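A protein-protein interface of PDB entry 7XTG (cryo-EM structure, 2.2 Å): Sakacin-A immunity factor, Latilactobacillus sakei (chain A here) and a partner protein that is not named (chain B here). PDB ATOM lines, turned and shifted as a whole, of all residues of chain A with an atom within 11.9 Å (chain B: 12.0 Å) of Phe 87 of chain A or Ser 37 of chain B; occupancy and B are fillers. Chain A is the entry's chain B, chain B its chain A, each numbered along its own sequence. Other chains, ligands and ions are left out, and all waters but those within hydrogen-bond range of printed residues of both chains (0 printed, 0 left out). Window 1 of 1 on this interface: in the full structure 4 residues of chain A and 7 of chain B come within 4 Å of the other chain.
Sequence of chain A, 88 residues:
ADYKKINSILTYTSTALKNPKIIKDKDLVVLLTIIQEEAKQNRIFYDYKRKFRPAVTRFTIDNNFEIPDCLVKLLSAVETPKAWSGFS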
ATOM      1  N   TYR A  48      -2.440  -1.846 -34.583  1.00  0.00           N
ATOM      2  CA  TYR A  48      -2.490  -2.548 -33.309  1.00  0.00           C
ATOM      3  C   TYR A  48      -3.922  -2.910 -32.954  1.00  0.00           C
ATOM      4  O   TYR A  48      -4.160  -3.915 -32.276  1.00  0.00           O
ATOM      5  CB  TYR A  48      -1.850  -1.697 -32.213  1.00  0.00           C
ATOM      6  CG  TYR A  48      -2.512  -0.355 -31.973  1.00  0.00           C
ATOM      7  CD1 TYR A  48      -2.285   0.719 -32.828  1.00  0.00           C
ATOM      8  CD2 TYR A  48      -3.327  -0.150 -30.871  1.00  0.00           C
ATOM      9  CE1 TYR A  48      -2.881   1.949 -32.609  1.00  0.00           C
ATOM     10  CE2 TYR A  48      -3.920   1.079 -30.638  1.00  0.00           C
ATOM     11  CZ  TYR A  48      -3.696   2.126 -31.512  1.00  0.00           C
ATOM     12  OH  TYR A  48      -4.283   3.353 -31.290  1.00  0.00           O
ATOM     13  N   LYS A  49      -4.883  -2.105 -33.402  1.00  0.00           N
ATOM     14  CA  LYS A  49      -6.287  -2.494 -33.424  1.00  0.00           C
ATOM     15  C   LYS A  49      -6.540  -3.207 -34.746  1.00  0.00           C
ATOM     16  O   LYS A  49      -6.533  -2.574 -35.807  1.00  0.00           O
ATOM     17  CB  LYS A  49      -7.203  -1.281 -33.293  1.00  0.00           C
ATOM     18  CG  LYS A  49      -6.724  -0.194 -32.351  1.00  0.00           C
ATOM     19  CD  LYS A  49      -7.605   1.045 -32.467  1.00  0.00           C
ATOM     20  CE  LYS A  49      -7.244   2.089 -31.429  1.00  0.00           C
ATOM     21  NZ  LYS A  49      -8.218   3.217 -31.427  1.00  0.00           N
ATOM     22  N   ARG A  50      -6.756  -4.521 -34.687  1.00  0.00           N
ATOM     23  CA  ARG A  50      -6.945  -5.336 -35.889  1.00  0.00           C
ATOM     24  C   ARG A  50      -8.336  -5.064 -36.453  1.00  0.00           C
ATOM     25  O   ARG A  50      -9.278  -5.839 -36.281  1.00  0.00           O
ATOM     26  CB  ARG A  50      -6.766  -6.815 -35.572  1.00  0.00           C
ATOM     27  CG  ARG A  50      -5.375  -7.203 -35.113  1.00  0.00           C
ATOM     28  CD  ARG A  50      -5.446  -8.371 -34.155  1.00  0.00           C
ATOM     29  NE  ARG A  50      -5.737  -7.919 -32.801  1.00  0.00           N
ATOM     30  CZ  ARG A  50      -5.946  -8.728 -31.773  1.00  0.00           C
ATOM     31  NH1 ARG A  50      -5.907 -10.042 -31.912  1.00  0.00           N
ATOM     32  NH2 ARG A  50      -6.202  -8.207 -30.577  1.00  0.00           N
ATOM     33  N   LYS A  51      -8.458  -3.943 -37.160  1.00  0.00           N
ATOM     34  CA  LYS A  51      -9.746  -3.480 -37.659  1.00  0.00           C
ATOM     35  C   LYS A  51      -9.972  -3.770 -39.136  1.00  0.00           C
ATOM     36  O   LYS A  51     -11.120  -3.952 -39.545  1.00  0.00           O
ATOM     37  CB  LYS A  51      -9.885  -1.968 -37.421  1.00  0.00           C
ATOM     38  CG  LYS A  51      -9.678  -1.540 -35.970  1.00  0.00           C
ATOM     39  CD  LYS A  51     -10.936  -1.683 -35.130  1.00  0.00           C
ATOM     40  CE  LYS A  51     -10.977  -0.645 -34.004  1.00  0.00           C
ATOM     41  NZ  LYS A  51     -11.960   0.443 -34.262  1.00  0.00           N
ATOM     42  N   PRO A  54     -11.333  -7.721 -40.102  1.00  0.00           N
ATOM     43  CA  PRO A  54     -12.750  -7.909 -39.751  1.00  0.00           C
ATOM     44  C   PRO A  54     -13.671  -7.035 -40.583  1.00  0.00           C
ATOM     45  O   PRO A  54     -14.792  -7.444 -40.908  1.00  0.00           O
ATOM     46  CB  PRO A  54     -12.797  -7.540 -38.261  1.00  0.00           C
ATOM     47  CG  PRO A  54     -11.409  -7.729 -37.777  1.00  0.00           C
ATOM     48  CD  PRO A  54     -10.507  -7.413 -38.919  1.00  0.00           C
ATOM     49  N   ARG A  58     -16.768  -8.038 -42.930  1.00  0.00           N
ATOM     50  CA  ARG A  58     -18.075  -7.397 -42.826  1.00  0.00           C
ATOM     51  C   ARG A  58     -18.577  -6.950 -44.192  1.00  0.00           C
ATOM     52  O   ARG A  58     -19.733  -7.202 -44.555  1.00  0.00           O
ATOM     53  CB  ARG A  58     -17.980  -6.203 -41.875  1.00  0.00           C
ATOM     54  CG  ARG A  58     -19.184  -5.987 -40.970  1.00  0.00           C
ATOM     55  CD  ARG A  58     -18.938  -4.819 -40.014  1.00  0.00           C
ATOM     56  NE  ARG A  58     -17.516  -4.623 -39.746  1.00  0.00           N
ATOM     57  CZ  ARG A  58     -16.796  -5.366 -38.917  1.00  0.00           C
ATOM     58  NH1 ARG A  58     -17.333  -6.369 -38.241  1.00  0.00           N
ATOM     59  NH2 ARG A  58     -15.504  -5.095 -38.762  1.00  0.00           N
ATOM     60  N   ALA A  83       3.306 -10.833 -31.099  1.00  0.00           N
ATOM     61  CA  ALA A  83       4.050 -11.269 -29.913  1.00  0.00           C
ATOM     62  C   ALA A  83       3.118 -11.542 -28.731  1.00  0.00           C
ATOM     63  O   ALA A  83       3.301 -11.010 -27.636  1.00  0.00           O
ATOM     64  CB  ALA A  83       5.120 -10.250 -29.533  1.00  0.00           C
ATOM     65  N   TRP A  84       2.081 -12.358 -28.955  1.00  0.00           N
ATOM     66  CA  TRP A  84       1.087 -12.712 -27.938  1.00  0.00           C
ATOM     67  C   TRP A  84       1.678 -13.095 -26.582  1.00  0.00           C
ATOM     68  O   TRP A  84       2.757 -13.693 -26.512  1.00  0.00           O
ATOM     69  CB  TRP A  84       0.221 -13.876 -28.441  1.00  0.00           C
ATOM     70  CG  TRP A  84      -1.060 -14.124 -27.672  1.00  0.00           C
ATOM     71  CD1 TRP A  84      -1.608 -15.340 -27.383  1.00  0.00           C
ATOM     72  CD2 TRP A  84      -1.960 -13.148 -27.130  1.00  0.00           C
ATOM     73  NE1 TRP A  84      -2.779 -15.185 -26.683  1.00  0.00           N
ATOM     74  CE2 TRP A  84      -3.019 -13.848 -26.516  1.00  0.00           C
ATOM     75  CE3 TRP A  84      -1.971 -11.750 -27.096  1.00  0.00           C
ATOM     76  CZ2 TRP A  84      -4.071 -13.201 -25.876  1.00  0.00           C
ATOM     77  CZ3 TRP A  84      -3.016 -11.112 -26.462  1.00  0.00           C
ATOM     78  CH2 TRP A  84      -4.051 -11.837 -25.861  1.00  0.00           C
ATOM     79  N   SER A  85       0.964 -12.756 -25.502  1.00  0.00           N
ATOM     80  CA  SER A  85       1.315 -13.177 -24.151  1.00  0.00           C
ATOM     81  C   SER A  85       0.309 -14.132 -23.522  1.00  0.00           C
ATOM     82  O   SER A  85       0.715 -15.016 -22.762  1.00  0.00           O
ATOM     83  CB  SER A  85       1.471 -11.957 -23.232  1.00  0.00           C
ATOM     84  OG  SER A  85       0.956 -12.219 -21.937  1.00  0.00           O
ATOM     85  N   GLY A  86      -0.975 -13.987 -23.817  1.00  0.00           N
ATOM     86  CA  GLY A  86      -1.996 -14.894 -23.337  1.00  0.00           C
ATOM     87  C   GLY A  86      -2.903 -14.249 -22.303  1.00  0.00           C
ATOM     88  O   GLY A  86      -2.808 -13.058 -21.992  1.00  0.00           O
ATOM     89  N   PHE A  87      -3.810 -15.070 -21.774  1.00  0.00           N
ATOM     90  CA  PHE A  87      -4.784 -14.653 -20.772  1.00  0.00           C
ATOM     91  C   PHE A  87      -4.455 -15.178 -19.384  1.00  0.00           C
ATOM     92  O   PHE A  87      -4.720 -14.498 -18.390  1.00  0.00           O
ATOM     93  CB  PHE A  87      -6.188 -15.111 -21.193  1.00  0.00           C
ATOM     94  CG  PHE A  87      -6.802 -14.253 -22.262  1.00  0.00           C
ATOM     95  CD1 PHE A  87      -6.696 -12.872 -22.200  1.00  0.00           C
ATOM     96  CD2 PHE A  87      -7.469 -14.821 -23.335  1.00  0.00           C
ATOM     97  CE1 PHE A  87      -7.246 -12.075 -23.183  1.00  0.00           C
ATOM     98  CE2 PHE A  87      -8.030 -14.025 -24.320  1.00  0.00           C
ATOM     99  CZ  PHE A  87      -7.915 -12.650 -24.243  1.00  0.00           C
ATOM    100  N   SER A  88      -3.892 -16.381 -19.295  1.00  0.00           N
ATOM    101  CA  SER A  88      -3.404 -16.947 -18.037  1.00  0.00           C
ATOM    102  C   SER A  88      -4.486 -16.995 -16.958  1.00  0.00           C
ATOM    103  O   SER A  88      -5.431 -17.781 -17.037  1.00  0.00           O
ATOM    104  CB  SER A  88      -2.193 -16.152 -17.532  1.00  0.00           C
ATOM    105  OG  SER A  88      -1.507 -16.851 -16.507  1.00  0.00           O
ATOM    106  N   TYR B   5       4.110 -18.335 -10.109  1.00  0.00           N
ATOM    107  CA  TYR B   5       4.230 -18.544 -11.549  1.00  0.00           C
ATOM    108  C   TYR B   5       2.875 -18.655 -12.237  1.00  0.00           C
ATOM    109  O   TYR B   5       2.817 -19.023 -13.416  1.00  0.00           O
ATOM    110  CB  TYR B   5       5.073 -19.786 -11.861  1.00  0.00           C
ATOM    111  CG  TYR B   5       6.571 -19.577 -11.740  1.00  0.00           C
ATOM    112  CD1 TYR B   5       7.215 -18.594 -12.479  1.00  0.00           C
ATOM    113  CD2 TYR B   5       7.337 -20.365 -10.895  1.00  0.00           C
ATOM    114  CE1 TYR B   5       8.574 -18.395 -12.374  1.00  0.00           C
ATOM    115  CE2 TYR B   5       8.699 -20.175 -10.783  1.00  0.00           C
ATOM    116  CZ  TYR B   5       9.312 -19.188 -11.524  1.00  0.00           C
ATOM    117  OH  TYR B   5      10.669 -18.994 -11.419  1.00  0.00           O
ATOM    118  N   GLY B   6       1.791 -18.370 -11.528  1.00  0.00           N
ATOM    119  CA  GLY B   6       0.486 -18.239 -12.137  1.00  0.00           C
ATOM    120  C   GLY B   6      -0.189 -19.574 -12.407  1.00  0.00           C
ATOM    121  O   GLY B   6       0.417 -20.644 -12.337  1.00  0.00           O
ATOM    122  N   ASN B   7      -1.483 -19.490 -12.722  1.00  0.00           N
ATOM    123  CA  ASN B   7      -2.312 -20.637 -13.084  1.00  0.00           C
ATOM    124  C   ASN B   7      -2.364 -21.691 -11.982  1.00  0.00           C
ATOM    125  O   ASN B   7      -2.647 -22.861 -12.250  1.00  0.00           O
ATOM    126  CB  ASN B   7      -1.836 -21.254 -14.402  1.00  0.00           C
ATOM    127  CG  ASN B   7      -2.376 -20.522 -15.619  1.00  0.00           C
ATOM    128  OD1 ASN B   7      -3.563 -20.212 -15.692  1.00  0.00           O
ATOM    129  ND2 ASN B   7      -1.495 -20.206 -16.562  1.00  0.00           N
ATOM    130  N   GLY B   8      -2.092 -21.297 -10.739  1.00  0.00           N
ATOM    131  CA  GLY B   8      -2.196 -22.186  -9.603  1.00  0.00           C
ATOM    132  C   GLY B   8      -0.891 -22.709  -9.039  1.00  0.00           C
ATOM    133  O   GLY B   8      -0.857 -23.077  -7.858  1.00  0.00           O
ATOM    134  N   GLU B  22      -6.830 -21.556  -7.646  1.00  0.00           N
ATOM    135  CA  GLU B  22      -6.305 -20.586  -8.600  1.00  0.00           C
ATOM    136  C   GLU B  22      -6.262 -21.162 -10.008  1.00  0.00           C
ATOM    137  O   GLU B  22      -6.478 -20.429 -10.976  1.00  0.00           O
ATOM    138  CB  GLU B  22      -4.913 -20.110  -8.183  1.00  0.00           C
ATOM    139  CG  GLU B  22      -4.528 -18.770  -8.802  1.00  0.00           C
ATOM    140  CD  GLU B  22      -3.082 -18.719  -9.256  1.00  0.00           C
ATOM    141  OE1 GLU B  22      -2.847 -18.387 -10.437  1.00  0.00           O
ATOM    142  OE2 GLU B  22      -2.183 -19.013  -8.443  1.00  0.00           O
ATOM    143  N   ALA B  23      -5.999 -22.465 -10.145  1.00  0.00           N
ATOM    144  CA  ALA B  23      -6.105 -23.102 -11.454  1.00  0.00           C
ATOM    145  C   ALA B  23      -7.526 -22.999 -11.999  1.00  0.00           C
ATOM    146  O   ALA B  23      -7.725 -22.688 -13.179  1.00  0.00           O
ATOM    147  CB  ALA B  23      -5.659 -24.563 -11.363  1.00  0.00           C
ATOM    148  N   THR B  24      -8.525 -23.231 -11.142  1.00  0.00           N
ATOM    149  CA  THR B  24      -9.920 -23.117 -11.563  1.00  0.00           C
ATOM    150  C   THR B  24     -10.263 -21.689 -11.975  1.00  0.00           C
ATOM    151  O   THR B  24     -10.893 -21.465 -13.019  1.00  0.00           O
ATOM    152  CB  THR B  24     -10.847 -23.571 -10.433  1.00  0.00           C
ATOM    153  OG1 THR B  24     -10.292 -24.721  -9.782  1.00  0.00           O
ATOM    154  CG2 THR B  24     -12.221 -23.928 -10.977  1.00  0.00           C
ATOM    155  N   GLN B  25      -9.863 -20.709 -11.158  1.00  0.00           N
ATOM    156  CA  GLN B  25     -10.146 -19.313 -11.483  1.00  0.00           C
ATOM    157  C   GLN B  25      -9.475 -18.912 -12.789  1.00  0.00           C
ATOM    158  O   GLN B  25     -10.083 -18.232 -13.625  1.00  0.00           O
ATOM    159  CB  GLN B  25      -9.697 -18.386 -10.350  1.00  0.00           C
ATOM    160  CG  GLN B  25     -10.316 -18.630  -8.969  1.00  0.00           C
ATOM    161  CD  GLN B  25     -11.560 -19.505  -8.992  1.00  0.00           C
ATOM    162  OE1 GLN B  25     -12.653 -19.047  -9.334  1.00  0.00           O
ATOM    163  NE2 GLN B  25     -11.401 -20.769  -8.610  1.00  0.00           N
ATOM    164  N   SER B  26      -8.220 -19.320 -12.983  1.00  0.00           N
ATOM    165  CA  SER B  26      -7.525 -18.988 -14.219  1.00  0.00           C
ATOM    166  C   SER B  26      -8.189 -19.641 -15.423  1.00  0.00           C
ATOM    167  O   SER B  26      -8.314 -19.011 -16.477  1.00  0.00           O
ATOM    168  CB  SER B  26      -6.054 -19.385 -14.124  1.00  0.00           C
ATOM    169  OG  SER B  26      -5.406 -18.697 -13.068  1.00  0.00           O
ATOM    170  N   ILE B  27      -8.636 -20.893 -15.292  1.00  0.00           N
ATOM    171  CA  ILE B  27      -9.267 -21.545 -16.435  1.00  0.00           C
ATOM    172  C   ILE B  27     -10.581 -20.851 -16.787  1.00  0.00           C
ATOM    173  O   ILE B  27     -10.880 -20.621 -17.965  1.00  0.00           O
ATOM    174  CB  ILE B  27      -9.441 -23.058 -16.176  1.00  0.00           C
ATOM    175  CG1 ILE B  27      -9.525 -23.823 -17.493  1.00  0.00           C
ATOM    176  CG2 ILE B  27     -10.677 -23.375 -15.358  1.00  0.00           C
ATOM    177  CD1 ILE B  27      -8.762 -25.111 -17.448  1.00  0.00           C
ATOM    178  N   ILE B  28     -11.358 -20.449 -15.776  1.00  0.00           N
ATOM    179  CA  ILE B  28     -12.635 -19.793 -16.056  1.00  0.00           C
ATOM    180  C   ILE B  28     -12.413 -18.407 -16.660  1.00  0.00           C
ATOM    181  O   ILE B  28     -13.092 -18.013 -17.620  1.00  0.00           O
ATOM    182  CB  ILE B  28     -13.505 -19.744 -14.784  1.00  0.00           C
ATOM    183  CG1 ILE B  28     -14.215 -21.089 -14.590  1.00  0.00           C
ATOM    184  CG2 ILE B  28     -14.487 -18.583 -14.841  1.00  0.00           C
ATOM    185  CD1 ILE B  28     -14.733 -21.328 -13.197  1.00  0.00           C
ATOM    186  N   GLY B  29     -11.458 -17.649 -16.115  1.00  0.00           N
ATOM    187  CA  GLY B  29     -11.160 -16.340 -16.672  1.00  0.00           C
ATOM    188  C   GLY B  29     -10.600 -16.409 -18.079  1.00  0.00           C
ATOM    189  O   GLY B  29     -10.926 -15.575 -18.927  1.00  0.00           O
ATOM    190  N   GLY B  30      -9.744 -17.396 -18.348  1.00  0.00           N
ATOM    191  CA  GLY B  30      -9.272 -17.596 -19.705  1.00  0.00           C
ATOM    192  C   GLY B  30     -10.398 -17.950 -20.650  1.00  0.00           C
ATOM    193  O   GLY B  30     -10.439 -17.478 -21.788  1.00  0.00           O
ATOM    194  N   MET B  31     -11.332 -18.784 -20.190  1.00  0.00           N
ATOM    195  CA  MET B  31     -12.494 -19.113 -21.006  1.00  0.00           C
ATOM    196  C   MET B  31     -13.279 -17.858 -21.368  1.00  0.00           C
ATOM    197  O   MET B  31     -13.606 -17.628 -22.543  1.00  0.00           O
ATOM    198  CB  MET B  31     -13.380 -20.109 -20.262  1.00  0.00           C
ATOM    199  CG  MET B  31     -13.936 -21.212 -21.130  1.00  0.00           C
ATOM    200  SD  MET B  31     -15.407 -20.637 -21.996  1.00  0.00           S
ATOM    201  CE  MET B  31     -16.422 -20.080 -20.631  1.00  0.00           C
ATOM    202  N   ILE B  32     -13.565 -17.017 -20.369  1.00  0.00           N
ATOM    203  CA  ILE B  32     -14.335 -15.799 -20.621  1.00  0.00           C
ATOM    204  C   ILE B  32     -13.580 -14.875 -21.568  1.00  0.00           C
ATOM    205  O   ILE B  32     -14.154 -14.327 -22.519  1.00  0.00           O
ATOM    206  CB  ILE B  32     -14.672 -15.088 -19.298  1.00  0.00           C
ATOM    207  CG1 ILE B  32     -15.473 -16.011 -18.384  1.00  0.00           C
ATOM    208  CG2 ILE B  32     -15.462 -13.825 -19.572  1.00  0.00           C
ATOM    209  CD1 ILE B  32     -15.493 -15.561 -16.933  1.00  0.00           C
ATOM    210  N   SER B  33     -12.281 -14.680 -21.318  1.00  0.00           N
ATOM    211  CA  SER B  33     -11.504 -13.749 -22.130  1.00  0.00           C
ATOM    212  C   SER B  33     -11.413 -14.224 -23.572  1.00  0.00           C
ATOM    213  O   SER B  33     -11.617 -13.440 -24.506  1.00  0.00           O
ATOM    214  CB  SER B  33     -10.105 -13.578 -21.540  1.00  0.00           C
ATOM    215  OG  SER B  33     -10.128 -13.636 -20.129  1.00  0.00           O
ATOM    216  N   GLY B  34     -11.108 -15.506 -23.775  1.00  0.00           N
ATOM    217  CA  GLY B  34     -11.026 -16.029 -25.124  1.00  0.00           C
ATOM    218  C   GLY B  34     -12.346 -15.939 -25.861  1.00  0.00           C
ATOM    219  O   GLY B  34     -12.383 -15.545 -27.028  1.00  0.00           O
ATOM    220  N   TRP B  35     -13.450 -16.273 -25.186  1.00  0.00           N
ATOM    221  CA  TRP B  35     -14.748 -16.201 -25.846  1.00  0.00           C
ATOM    222  C   TRP B  35     -15.085 -14.770 -26.239  1.00  0.00           C
ATOM    223  O   TRP B  35     -15.462 -14.500 -27.387  1.00  0.00           O
ATOM    224  CB  TRP B  35     -15.819 -16.788 -24.934  1.00  0.00           C
ATOM    225  CG  TRP B  35     -16.358 -18.095 -25.423  1.00  0.00           C
ATOM    226  CD1 TRP B  35     -16.013 -19.336 -24.979  1.00  0.00           C
ATOM    227  CD2 TRP B  35     -17.344 -18.294 -26.444  1.00  0.00           C
ATOM    228  NE1 TRP B  35     -16.718 -20.300 -25.660  1.00  0.00           N
ATOM    229  CE2 TRP B  35     -17.544 -19.685 -26.563  1.00  0.00           C
ATOM    230  CE3 TRP B  35     -18.074 -17.434 -27.272  1.00  0.00           C
ATOM    231  CZ2 TRP B  35     -18.442 -20.235 -27.474  1.00  0.00           C
ATOM    232  CZ3 TRP B  35     -18.966 -17.982 -28.177  1.00  0.00           C
ATOM    233  CH2 TRP B  35     -19.146 -19.368 -28.267  1.00  0.00           C
ATOM    234  N   ALA B  36     -14.936 -13.829 -25.303  1.00  0.00           N
ATOM    235  CA  ALA B  36     -15.287 -12.441 -25.586  1.00  0.00           C
ATOM    236  C   ALA B  36     -14.408 -11.861 -26.688  1.00  0.00           C
ATOM    237  O   ALA B  36     -14.900 -11.178 -27.592  1.00  0.00           O
ATOM    238  CB  ALA B  36     -15.183 -11.602 -24.314  1.00  0.00           C
ATOM    239  N   SER B  37     -13.100 -12.125 -26.630  1.00  0.00           N
ATOM    240  CA  SER B  37     -12.198 -11.601 -27.648  1.00  0.00           C
ATOM    241  C   SER B  37     -12.470 -12.216 -29.014  1.00  0.00           C
ATOM    242  O   SER B  37     -12.451 -11.506 -30.021  1.00  0.00           O
ATOM    243  CB  SER B  37     -10.748 -11.831 -27.231  1.00  0.00           C
ATOM    244  OG  SER B  37     -10.610 -13.055 -26.530  1.00  0.00           O
ATOM    245  N   GLY B  38     -12.708 -13.528 -29.080  1.00  0.00           N
ATOM    246  CA  GLY B  38     -13.031 -14.137 -30.358  1.00  0.00           C
ATOM    247  C   GLY B  38     -14.337 -13.624 -30.930  1.00  0.00           C
ATOM    248  O   GLY B  38     -14.478 -13.463 -32.144  1.00  0.00           O
ATOM    249  N   LEU B  39     -15.310 -13.348 -30.060  1.00  0.00           N
ATOM    250  CA  LEU B  39     -16.588 -12.830 -30.530  1.00  0.00           C
ATOM    251  C   LEU B  39     -16.470 -11.383 -30.994  1.00  0.00           C
ATOM    252  O   LEU B  39     -17.117 -10.993 -31.972  1.00  0.00           O
ATOM    253  CB  LEU B  39     -17.633 -12.964 -29.423  1.00  0.00           C
ATOM    254  CG  LEU B  39     -18.191 -14.369 -29.200  1.00  0.00           C
ATOM    255  CD1 LEU B  39     -19.410 -14.316 -28.301  1.00  0.00           C
ATOM    256  CD2 LEU B  39     -18.528 -15.044 -30.524  1.00  0.00           C
ATOM    257  N   ALA B  40     -15.654 -10.575 -30.312  1.00  0.00           N
ATOM    258  CA  ALA B  40     -15.493  -9.174 -30.683  1.00  0.00           C
ATOM    259  C   ALA B  40     -14.562  -8.983 -31.876  1.00  0.00           C
ATOM    260  O   ALA B  40     -14.758  -8.050 -32.662  1.00  0.00           O
ATOM    261  CB  ALA B  40     -14.977  -8.373 -29.486  1.00  0.00           C
ATOM    262  N   GLY B  41     -13.549  -9.838 -32.023  1.00  0.00           N
ATOM    263  CA  GLY B  41     -12.577  -9.651 -33.088  1.00  0.00           C
ATOM    264  C   GLY B  41     -13.189  -9.784 -34.468  1.00  0.00           C
ATOM    265  O   GLY B  41     -12.668  -9.237 -35.441  1.00  0.00           O
ATOM    266  N   MET B  42     -14.290 -10.514 -34.570  1.00  0.00           N
ATOM    267  CA  MET B  42     -14.997 -10.703 -35.829  1.00  0.00           C
ATOM    268  C   MET B  42     -16.023  -9.597 -36.076  1.00  0.00           C
ATOM    269  O   MET B  42     -16.252  -9.193 -37.220  1.00  0.00           O
ATOM    270  CB  MET B  42     -15.662 -12.084 -35.838  1.00  0.00           C
ATOM    271  CG  MET B  42     -16.851 -12.221 -36.755  1.00  0.00           C
ATOM    272  SD  MET B  42     -18.385 -11.764 -35.919  1.00  0.00           S
ATOM    273  CE  MET B  42     -18.249 -12.713 -34.406  1.00  0.00           C
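Pro 54 of chain A touches Gly 41 of chain B. Met 42 of chain B touches Pro 54 of chain A. Phe 87 of chain A touches Ser 33 of chain B (CD2 to CB, 3.4 Å). Phe 87 of chain A touches Gly 34 of chain B. Phe 87 of chain A touches Ser 37 of chain B.
Of the printed residues of chain B, Pro 54 of chain A touches Gly 41 (3.1 Å) and Met 42 (3.97 Å). Printed residues of chain B within 4 Å of Arg 58 of chain A: Met 42. No residue of chain B comes within 4 Å of Gly 86 of chain A. Phe 87 of chain A touches just these residues of chain B: Ser 33 (3.4 Å), Gly 34 (3.5 Å) and Ser 37 (3.5 Å). Printed residues of chain A within 4 Å of Asn 7 of chain B: Ser 88. Ala 23 of chain B touches none of the printed residues of chain A. Of the printed residues of chain A, Ser 26 of chain B touches Ser 88. No residue of chain A comes within 4 Å of Gly 29 of chain B. No residue of chain A comes within 4 Å of Gly 30 of chain B. Of chain A, only Phe 87 (3.5 Å) comes within 4 Å of Ser 37 of chain B. No residue of chain A comes within 4 Å of Leu 39 of chain B. Ala 40 of chain B touches none of the printed residues of chain A. Printed residues of chain A within 4 Å of Met 42 of chain B: Pro 54 (3.97 Å) and Arg 58 (3.2 Å). The nearest residue of chain B that does not touch Phe 87 of chain A is Gly 30 of chain B (4.2 Å). The nearest printed residue of chain A that does not touch Ser 26 of chain B is Phe 87 of chain A (6.1 Å).
Of the 12 printed residues of chain A, 4 touch a printed residue of chain B. Printed residues of chain B that touch a printed residue of chain A: Asn 7, Ser 26, Ser 33, Gly 34, Ser 37, Gly 41 and Met 42. Among the printed residues, 8 pairs touch across the chains. Among the printed residues, no Asp or Glu carboxylate lies within 4 Å of a Lys or Arg side-chain nitrogen of the other chain.
The backbone NH (N) of Asn 7 of chain B sits at hydrogen-bond distance from the side-chain carboxylate (OE1) of Glu 22 of chain B (2.9 Å). O of Glu 22 of chain B lies within hydrogen-bond range of OG of Ser 26 of chain B (2.9 Å). The backbone carbonyl oxygen (O) of Gly 29 of chain B sits at hydrogen-bond distance from the side-chain hydroxyl (OG) of Ser 33 of chain B, 2.4 Å away. The backbone carbonyl oxygen (O) of Gly 34 of chain B is in hydrogen-bond range of the side-chain hydroxyl (OG) of Ser 37 of chain B. The guanidinium group (NH2) of Arg 58 of chain A lies close to the backbone carbonyl oxygen (O) of Pro 54 of chain A, 3.3 Å away.
O of Ser 88 of chain A lies close to OD1 of Asn 7 of chain B. The guanidinium group (NH1) of Arg 58 of chain A is in hydrogen-bond range of the backbone carbonyl oxygen (O) of Met 42 of chain B, 3.2 Å away. The backbone carbonyl oxygen of Ser 88 of chain A sits close to the backbone carbonyl oxygen of Ser 26 of chain B (3.2 Å).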
